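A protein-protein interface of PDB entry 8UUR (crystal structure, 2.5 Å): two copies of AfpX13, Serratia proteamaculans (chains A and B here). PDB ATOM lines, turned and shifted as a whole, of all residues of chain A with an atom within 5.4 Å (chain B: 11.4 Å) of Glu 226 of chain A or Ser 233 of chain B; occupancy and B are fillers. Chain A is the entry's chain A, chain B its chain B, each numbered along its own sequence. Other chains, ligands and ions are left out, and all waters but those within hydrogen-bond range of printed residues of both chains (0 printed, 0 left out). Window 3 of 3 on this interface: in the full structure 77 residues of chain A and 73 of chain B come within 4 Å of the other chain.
Among the printed residues, merely in contact across the chains: Glu 226 of chain A with Ser 233 of chain B, Glu 226 of chain A with Leu 262 of chain B, Ile 227 of chain A with Gly 232 of chain B, Ile 228 of chain A with Met 230 of chain B, Ile 228 of chain A with Val 231 of chain B, Ile 228 of chain A with Ile 236 of chain B, Ile 228 of chain A with Leu 262 of chain B, Met 241 of chain A with Gly 207 of chain B, Ser 243 of chain A with Leu 262 of chain B, Ser 243 of chain A with Ile 263 of chain B and Lys 245 of chain A with Ile 263 of chain B.
Of the 20 printed residues of chain B, 8 touch a printed residue of chain A.
Hydrophobic or aromatic side chains of chain B within 4 Å of the printed part of chain A: Met 230, Ile 236, Leu 262 and Ile 263.
Of the 9 printed residues of chain A, 6 touch a printed residue of chain B.
Hydrophobic or aromatic side chains of chain A within 4 Å of the printed part of chain B: Ile 228 and Met 241.
Among the printed residues, 11 pairs touch across the chains.
No position is printed for both chains.
Of chain B, only Ser 233 and Leu 262 come within 4 Å of Glu 226 of chain A.
Ser 233 of chain B touches one residue of chain A.
No residue of chain B comes within 4 Å of His 224 of chain A.
No residue of chain B comes within 4 Å of Asn 225 of chain A.
Ile 227 of chain A touches just one residue of chain B: Gly 232.
Of chain B, only Met 230 (3.6 Å), Val 231 (3.6 Å), Ile 236 (3.9 Å) and Leu 262 (3.7 Å) come within 4 Å of Ile 228 of chain A.
No residue of chain B comes within 4 Å of Val 242 of chain A.
Ser 243 of chain A touches just these residues of chain B: Leu 262 and Ile 263.
Printed residues of chain A within 4 Å of Val 231 of chain B: Ile 228.
Of the printed residues of chain A, Gly 207 of chain B touches Met 241 (3.7 Å).
Of the printed residues of chain A, Gly 232 of chain B touches Ile 227 (3.4 Å).
Thr 264 of chain B touches none of the printed residues of chain A.
The nearest residue of chain B that does not touch Glu 226 of chain A is Ile 236 of chain B (4.5 Å).
The nearest residue of chain A that does not touch Ser 233 of chain B is Ile 227 of chain A (4.1 Å).
O of Ser 243 of chain A sits at hydrogen-bond distance from N of Asn 225 of chain A, 2.7 Å away.
The side-chain amide oxygen of Asn 225 of chain A is in hydrogen-bond range of the backbone NH of Lys 245 of chain A (2.7 Å).
The backbone carbonyl oxygen (O) of Glu 226 of chain A is in hydrogen-bond range of the backbone NH (N) of Ser 243 of chain A, 2.8 Å away.
The backbone carbonyl oxygen of Met 230 of chain B lies within hydrogen-bond range of the backbone NH of Ala 238 of chain B (2.8 Å).
The backbone NH of Ile 263 of chain B sits at hydrogen-bond distance from the side-chain amide oxygen of Asn 261 of chain B, at 2.9 Å.
The backbone NH (N) of Ile 228 of chain A is in hydrogen-bond range of the backbone carbonyl oxygen (O) of Met 241 of chain A, at 2.7 Å.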
ATOM      1  N   HIS A 224       7.228  38.663   2.652  1.00  0.00           N
ATOM      2  CA  HIS A 224       7.659  37.524   3.443  1.00  0.00           C
ATOM      3  C   HIS A 224       6.797  36.299   3.143  1.00  0.00           C
ATOM      4  O   HIS A 224       5.676  36.403   2.648  1.00  0.00           O
ATOM      5  CB  HIS A 224       7.580  37.858   4.924  1.00  0.00           C
ATOM      6  CG  HIS A 224       6.184  37.878   5.478  1.00  0.00           C
ATOM      7  ND1 HIS A 224       5.390  39.006   5.465  1.00  0.00           N
ATOM      8  CD2 HIS A 224       5.449  36.915   6.087  1.00  0.00           C
ATOM      9  CE1 HIS A 224       4.229  38.739   6.037  1.00  0.00           C
ATOM     10  NE2 HIS A 224       4.238  37.475   6.421  1.00  0.00           N
ATOM     11  N   ASN A 225       7.338  35.123   3.461  1.00  0.00           N
ATOM     12  CA  ASN A 225       6.583  33.864   3.374  1.00  0.00           C
ATOM     13  C   ASN A 225       5.871  33.552   4.682  1.00  0.00           C
ATOM     14  O   ASN A 225       4.634  33.587   4.747  1.00  0.00           O
ATOM     15  CB  ASN A 225       7.526  32.723   2.992  1.00  0.00           C
ATOM     16  CG  ASN A 225       7.977  32.805   1.575  1.00  0.00           C
ATOM     17  OD1 ASN A 225       9.021  33.381   1.275  1.00  0.00           O
ATOM     18  ND2 ASN A 225       7.190  32.226   0.676  1.00  0.00           N
ATOM     19  N   GLU A 226       6.618  33.232   5.738  1.00  0.00           N
ATOM     20  CA  GLU A 226       6.072  32.844   7.028  1.00  0.00           C
ATOM     21  C   GLU A 226       6.511  33.846   8.086  1.00  0.00           C
ATOM     22  O   GLU A 226       7.537  34.521   7.951  1.00  0.00           O
ATOM     23  CB  GLU A 226       6.526  31.430   7.448  1.00  0.00           C
ATOM     24  CG  GLU A 226       6.449  30.361   6.352  1.00  0.00           C
ATOM     25  CD  GLU A 226       5.023  29.924   6.050  1.00  0.00           C
ATOM     26  OE1 GLU A 226       4.128  30.221   6.870  1.00  0.00           O
ATOM     27  OE2 GLU A 226       4.801  29.274   4.997  1.00  0.00           O
ATOM     28  N   ILE A 227       5.738  33.932   9.168  1.00  0.00           N
ATOM     29  CA  ILE A 227       6.065  34.869  10.231  1.00  0.00           C
ATOM     30  C   ILE A 227       5.559  34.305  11.547  1.00  0.00           C
ATOM     31  O   ILE A 227       4.616  33.517  11.572  1.00  0.00           O
ATOM     32  CB  ILE A 227       5.485  36.256   9.886  1.00  0.00           C
ATOM     33  CG1 ILE A 227       6.095  37.367  10.719  1.00  0.00           C
ATOM     34  CG2 ILE A 227       4.016  36.266  10.120  1.00  0.00           C
ATOM     35  CD1 ILE A 227       5.788  38.724  10.109  1.00  0.00           C
ATOM     36  N   ILE A 228       6.225  34.685  12.645  1.00  0.00           N
ATOM     37  CA  ILE A 228       5.906  34.227  13.997  1.00  0.00           C
ATOM     38  C   ILE A 228       5.766  35.443  14.899  1.00  0.00           C
ATOM     39  O   ILE A 228       6.596  36.358  14.838  1.00  0.00           O
ATOM     40  CB  ILE A 228       6.986  33.272  14.551  1.00  0.00           C
ATOM     41  CG1 ILE A 228       6.925  31.920  13.824  1.00  0.00           C
ATOM     42  CG2 ILE A 228       6.810  33.085  16.044  1.00  0.00           C
ATOM     43  CD1 ILE A 228       8.074  30.960  14.166  1.00  0.00           C
ATOM     44  N   MET A 241       9.534  36.851  14.257  1.00  0.00           N
ATOM     45  CA  MET A 241      10.378  36.113  13.347  1.00  0.00           C
ATOM     46  C   MET A 241       9.712  36.182  11.997  1.00  0.00           C
ATOM     47  O   MET A 241       8.518  35.898  11.900  1.00  0.00           O
ATOM     48  CB  MET A 241      10.538  34.665  13.784  1.00  0.00           C
ATOM     49  CG  MET A 241      11.498  34.485  14.902  1.00  0.00           C
ATOM     50  SD  MET A 241      11.616  32.734  15.259  1.00  0.00           S
ATOM     51  CE  MET A 241      12.760  32.249  13.968  1.00  0.00           C
ATOM     52  N   VAL A 242      10.480  36.560  10.976  1.00  0.00           N
ATOM     53  CA  VAL A 242       9.993  36.744   9.614  1.00  0.00           C
ATOM     54  C   VAL A 242      10.873  35.947   8.656  1.00  0.00           C
ATOM     55  O   VAL A 242      12.105  35.959   8.768  1.00  0.00           O
ATOM     56  CB  VAL A 242       9.986  38.235   9.217  1.00  0.00           C
ATOM     57  CG1 VAL A 242       9.194  38.424   7.966  1.00  0.00           C
ATOM     58  CG2 VAL A 242       9.385  39.079  10.311  1.00  0.00           C
ATOM     59  N   SER A 243      10.253  35.294   7.683  1.00  0.00           N
ATOM     60  CA  SER A 243      10.990  34.397   6.803  1.00  0.00           C
ATOM     61  C   SER A 243      10.707  34.716   5.339  1.00  0.00           C
ATOM     62  O   SER A 243       9.586  35.095   4.988  1.00  0.00           O
ATOM     63  CB  SER A 243      10.608  32.948   7.117  1.00  0.00           C
ATOM     64  OG  SER A 243      11.589  32.051   6.668  1.00  0.00           O
ATOM     65  N   LYS A 245      11.447  32.438   1.882  1.00  0.00           N
ATOM     66  CA  LYS A 245      11.914  31.143   1.395  1.00  0.00           C
ATOM     67  C   LYS A 245      13.033  31.275   0.369  1.00  0.00           C
ATOM     68  O   LYS A 245      13.920  30.418   0.304  1.00  0.00           O
ATOM     69  CB  LYS A 245      10.739  30.357   0.801  1.00  0.00           C
ATOM     70  CG  LYS A 245       9.720  29.943   1.856  1.00  0.00           C
ATOM     71  CD  LYS A 245       8.721  28.896   1.376  1.00  0.00           C
ATOM     72  CE  LYS A 245       8.082  28.137   2.562  1.00  0.00           C
ATOM     73  NZ  LYS A 245       6.739  28.665   3.009  1.00  0.00           N
ATOM     74  N   GLY B 207      18.271  31.296  12.134  1.00  0.00           N
ATOM     75  CA  GLY B 207      16.943  31.160  11.572  1.00  0.00           C
ATOM     76  C   GLY B 207      16.060  30.134  12.252  1.00  0.00           C
ATOM     77  O   GLY B 207      14.870  30.044  11.926  1.00  0.00           O
ATOM     78  N   TYR B 209      14.054  27.886  15.326  1.00  0.00           N
ATOM     79  CA  TYR B 209      13.267  28.099  16.524  1.00  0.00           C
ATOM     80  C   TYR B 209      13.039  26.756  17.200  1.00  0.00           C
ATOM     81  O   TYR B 209      13.155  25.697  16.572  1.00  0.00           O
ATOM     82  CB  TYR B 209      11.933  28.783  16.211  1.00  0.00           C
ATOM     83  CG  TYR B 209      10.917  27.916  15.466  1.00  0.00           C
ATOM     84  CD1 TYR B 209      10.039  27.087  16.172  1.00  0.00           C
ATOM     85  CD2 TYR B 209      10.808  27.960  14.055  1.00  0.00           C
ATOM     86  CE1 TYR B 209       9.097  26.322  15.523  1.00  0.00           C
ATOM     87  CE2 TYR B 209       9.834  27.193  13.379  1.00  0.00           C
ATOM     88  CZ  TYR B 209       8.992  26.373  14.130  1.00  0.00           C
ATOM     89  OH  TYR B 209       8.041  25.585  13.535  1.00  0.00           O
ATOM     90  N   MET B 212       7.732  23.272  20.521  1.00  0.00           N
ATOM     91  CA  MET B 212       7.075  23.245  21.816  1.00  0.00           C
ATOM     92  C   MET B 212       6.287  21.959  22.066  1.00  0.00           C
ATOM     93  O   MET B 212       5.716  21.798  23.150  1.00  0.00           O
ATOM     94  CB  MET B 212       6.180  24.481  21.961  1.00  0.00           C
ATOM     95  CG  MET B 212       5.403  24.814  20.730  1.00  0.00           C
ATOM     96  SD  MET B 212       4.006  23.696  20.454  1.00  0.00           S
ATOM     97  CE  MET B 212       2.927  24.172  21.815  1.00  0.00           C
ATOM     98  N   TYR B 213       6.269  21.032  21.109  1.00  0.00           N
ATOM     99  CA  TYR B 213       5.582  19.756  21.277  1.00  0.00           C
ATOM    100  C   TYR B 213       6.122  18.964  22.467  1.00  0.00           C
ATOM    101  O   TYR B 213       7.329  18.924  22.717  1.00  0.00           O
ATOM    102  CB  TYR B 213       5.737  18.917  20.009  1.00  0.00           C
ATOM    103  CG  TYR B 213       4.865  19.350  18.860  1.00  0.00           C
ATOM    104  CD1 TYR B 213       3.618  19.918  19.091  1.00  0.00           C
ATOM    105  CD2 TYR B 213       5.289  19.196  17.546  1.00  0.00           C
ATOM    106  CE1 TYR B 213       2.798  20.309  18.043  1.00  0.00           C
ATOM    107  CE2 TYR B 213       4.481  19.582  16.482  1.00  0.00           C
ATOM    108  CZ  TYR B 213       3.229  20.140  16.738  1.00  0.00           C
ATOM    109  OH  TYR B 213       2.408  20.545  15.701  1.00  0.00           O
ATOM    110  N   SER B 229       4.886  30.215  24.290  1.00  0.00           N
ATOM    111  CA  SER B 229       5.360  30.222  22.917  1.00  0.00           C
ATOM    112  C   SER B 229       4.918  31.482  22.210  1.00  0.00           C
ATOM    113  O   SER B 229       3.995  32.173  22.639  1.00  0.00           O
ATOM    114  CB  SER B 229       4.853  29.016  22.128  1.00  0.00           C
ATOM    115  OG  SER B 229       5.141  27.820  22.832  1.00  0.00           O
ATOM    116  N   MET B 230       5.617  31.774  21.123  1.00  0.00           N
ATOM    117  CA  MET B 230       5.125  32.666  20.091  1.00  0.00           C
ATOM    118  C   MET B 230       4.490  31.823  19.001  1.00  0.00           C
ATOM    119  O   MET B 230       4.888  30.677  18.777  1.00  0.00           O
ATOM    120  CB  MET B 230       6.261  33.509  19.536  1.00  0.00           C
ATOM    121  CG  MET B 230       7.159  34.017  20.631  1.00  0.00           C
ATOM    122  SD  MET B 230       8.320  35.249  20.067  1.00  0.00           S
ATOM    123  CE  MET B 230       9.657  34.281  19.388  1.00  0.00           C
ATOM    124  N   VAL B 231       3.462  32.371  18.369  1.00  0.00           N
ATOM    125  CA  VAL B 231       2.588  31.622  17.468  1.00  0.00           C
ATOM    126  C   VAL B 231       2.757  32.115  16.043  1.00  0.00           C
ATOM    127  O   VAL B 231       2.923  33.312  15.803  1.00  0.00           O
ATOM    128  CB  VAL B 231       1.123  31.716  17.918  1.00  0.00           C
ATOM    129  CG1 VAL B 231       0.925  30.918  19.186  1.00  0.00           C
ATOM    130  CG2 VAL B 231       0.819  33.173  18.242  1.00  0.00           C
ATOM    131  N   GLY B 232       2.771  31.173  15.111  1.00  0.00           N
ATOM    132  CA  GLY B 232       2.841  31.469  13.696  1.00  0.00           C
ATOM    133  C   GLY B 232       1.577  30.931  13.080  1.00  0.00           C
ATOM    134  O   GLY B 232       0.683  30.509  13.821  1.00  0.00           O
ATOM    135  N   SER B 233       1.473  30.921  11.755  1.00  0.00           N
ATOM    136  CA  SER B 233       0.227  30.513  11.119  1.00  0.00           C
ATOM    137  C   SER B 233       0.143  28.998  11.002  1.00  0.00           C
ATOM    138  O   SER B 233       1.137  28.319  10.724  1.00  0.00           O
ATOM    139  CB  SER B 233       0.090  31.146   9.735  1.00  0.00           C
ATOM    140  OG  SER B 233       0.776  30.376   8.769  1.00  0.00           O
ATOM    141  N   GLY B 234      -1.059  28.469  11.211  1.00  0.00           N
ATOM    142  CA  GLY B 234      -1.297  27.071  10.911  1.00  0.00           C
ATOM    143  C   GLY B 234      -0.493  26.144  11.790  1.00  0.00           C
ATOM    144  O   GLY B 234       0.293  25.326  11.297  1.00  0.00           O
ATOM    145  N   SER B 235      -0.670  26.294  13.099  1.00  0.00           N
ATOM    146  CA  SER B 235      -0.124  25.408  14.114  1.00  0.00           C
ATOM    147  C   SER B 235       1.381  25.518  14.249  1.00  0.00           C
ATOM    148  O   SER B 235       1.997  24.635  14.848  1.00  0.00           O
ATOM    149  CB  SER B 235      -0.496  23.946  13.844  1.00  0.00           C
ATOM    150  OG  SER B 235      -1.883  23.836  13.575  1.00  0.00           O
ATOM    151  N   ILE B 236       2.004  26.545  13.677  1.00  0.00           N
ATOM    152  CA  ILE B 236       3.405  26.806  13.965  1.00  0.00           C
ATOM    153  C   ILE B 236       3.466  27.561  15.283  1.00  0.00           C
ATOM    154  O   ILE B 236       2.677  28.489  15.520  1.00  0.00           O
ATOM    155  CB  ILE B 236       4.075  27.590  12.827  1.00  0.00           C
ATOM    156  CG1 ILE B 236       4.431  26.657  11.679  1.00  0.00           C
ATOM    157  CG2 ILE B 236       5.379  28.214  13.303  1.00  0.00           C
ATOM    158  CD1 ILE B 236       4.466  27.345  10.303  1.00  0.00           C
ATOM    159  N   ALA B 237       4.361  27.120  16.165  1.00  0.00           N
ATOM    160  CA  ALA B 237       4.544  27.722  17.476  1.00  0.00           C
ATOM    161  C   ALA B 237       5.993  27.488  17.881  1.00  0.00           C
ATOM    162  O   ALA B 237       6.557  26.418  17.618  1.00  0.00           O
ATOM    163  CB  ALA B 237       3.580  27.135  18.521  1.00  0.00           C
ATOM    164  N   ALA B 238       6.577  28.501  18.522  1.00  0.00           N
ATOM    165  CA  ALA B 238       7.998  28.555  18.843  1.00  0.00           C
ATOM    166  C   ALA B 238       8.169  28.764  20.343  1.00  0.00           C
ATOM    167  O   ALA B 238       7.743  29.792  20.876  1.00  0.00           O
ATOM    168  CB  ALA B 238       8.672  29.687  18.063  1.00  0.00           C
ATOM    169  N   LYS B 260      13.218  23.699  14.653  1.00  0.00           N
ATOM    170  CA  LYS B 260      12.488  23.796  13.391  1.00  0.00           C
ATOM    171  C   LYS B 260      12.771  25.152  12.750  1.00  0.00           C
ATOM    172  O   LYS B 260      13.497  25.980  13.299  1.00  0.00           O
ATOM    173  CB  LYS B 260      10.990  23.530  13.606  1.00  0.00           C
ATOM    174  CG  LYS B 260      10.746  22.117  14.141  1.00  0.00           C
ATOM    175  CD  LYS B 260       9.267  21.798  14.409  1.00  0.00           C
ATOM    176  CE  LYS B 260       9.063  20.281  14.580  1.00  0.00           C
ATOM    177  NZ  LYS B 260       7.726  19.816  14.130  1.00  0.00           N
ATOM    178  N   ASN B 261      12.223  25.374  11.559  1.00  0.00           N
ATOM    179  CA  ASN B 261      12.586  26.578  10.837  1.00  0.00           C
ATOM    180  C   ASN B 261      11.384  26.939   9.975  1.00  0.00           C
ATOM    181  O   ASN B 261      10.485  26.118   9.758  1.00  0.00           O
ATOM    182  CB  ASN B 261      13.891  26.323  10.051  1.00  0.00           C
ATOM    183  CG  ASN B 261      13.684  25.528   8.748  1.00  0.00           C
ATOM    184  OD1 ASN B 261      12.678  25.671   8.073  1.00  0.00           O
ATOM    185  ND2 ASN B 261      14.503  24.507   8.561  1.00  0.00           N
ATOM    186  N   LEU B 262      11.373  28.162   9.459  1.00  0.00           N
ATOM    187  CA  LEU B 262      10.203  28.616   8.720  1.00  0.00           C
ATOM    188  C   LEU B 262      10.286  28.359   7.216  1.00  0.00           C
ATOM    189  O   LEU B 262       9.300  28.609   6.515  1.00  0.00           O
ATOM    190  CB  LEU B 262       9.970  30.106   8.995  1.00  0.00           C
ATOM    191  CG  LEU B 262       9.526  30.365  10.442  1.00  0.00           C
ATOM    192  CD1 LEU B 262       9.340  31.839  10.735  1.00  0.00           C
ATOM    193  CD2 LEU B 262       8.252  29.584  10.767  1.00  0.00           C
ATOM    194  N   ILE B 263      11.407  27.838   6.704  1.00  0.00           N
ATOM    195  CA  ILE B 263      11.549  27.616   5.266  1.00  0.00           C
ATOM    196  C   ILE B 263      11.329  26.150   4.889  1.00  0.00           C
ATOM    197  O   ILE B 263      10.498  25.847   4.023  1.00  0.00           O
ATOM    198  CB  ILE B 263      12.915  28.091   4.740  1.00  0.00           C
ATOM    199  CG1 ILE B 263      13.061  29.606   4.853  1.00  0.00           C
ATOM    200  CG2 ILE B 263      13.054  27.723   3.273  1.00  0.00           C
ATOM    201  CD1 ILE B 263      14.514  30.067   4.702  1.00  0.00           C
ATOM    202  N   THR B 264      12.074  25.233   5.501  1.00  0.00           N
ATOM    203  CA  THR B 264      11.804  23.817   5.282  1.00  0.00           C
ATOM    204  C   THR B 264      10.976  23.254   6.422  1.00  0.00           C
ATOM    205  O   THR B 264      10.787  23.878   7.467  1.00  0.00           O
ATOM    206  CB  THR B 264      13.086  22.985   5.124  1.00  0.00           C
ATOM    207  OG1 THR B 264      13.692  22.763   6.415  1.00  0.00           O
ATOM    208  CG2 THR B 264      14.065  23.672   4.183  1.00  0.00           C
ATOM    209  N   SER B 265      10.470  22.048   6.199  1.00  0.00           N
ATOM    210  CA  SER B 265       9.706  21.341   7.213  1.00  0.00           C
ATOM    211  C   SER B 265      10.560  20.374   8.025  1.00  0.00           C
ATOM    212  O   SER B 265      10.019  19.635   8.844  1.00  0.00           O
ATOM    213  CB  SER B 265       8.556  20.584   6.547  1.00  0.00           C
ATOM    214  OG  SER B 265       9.065  19.781   5.488  1.00  0.00           O
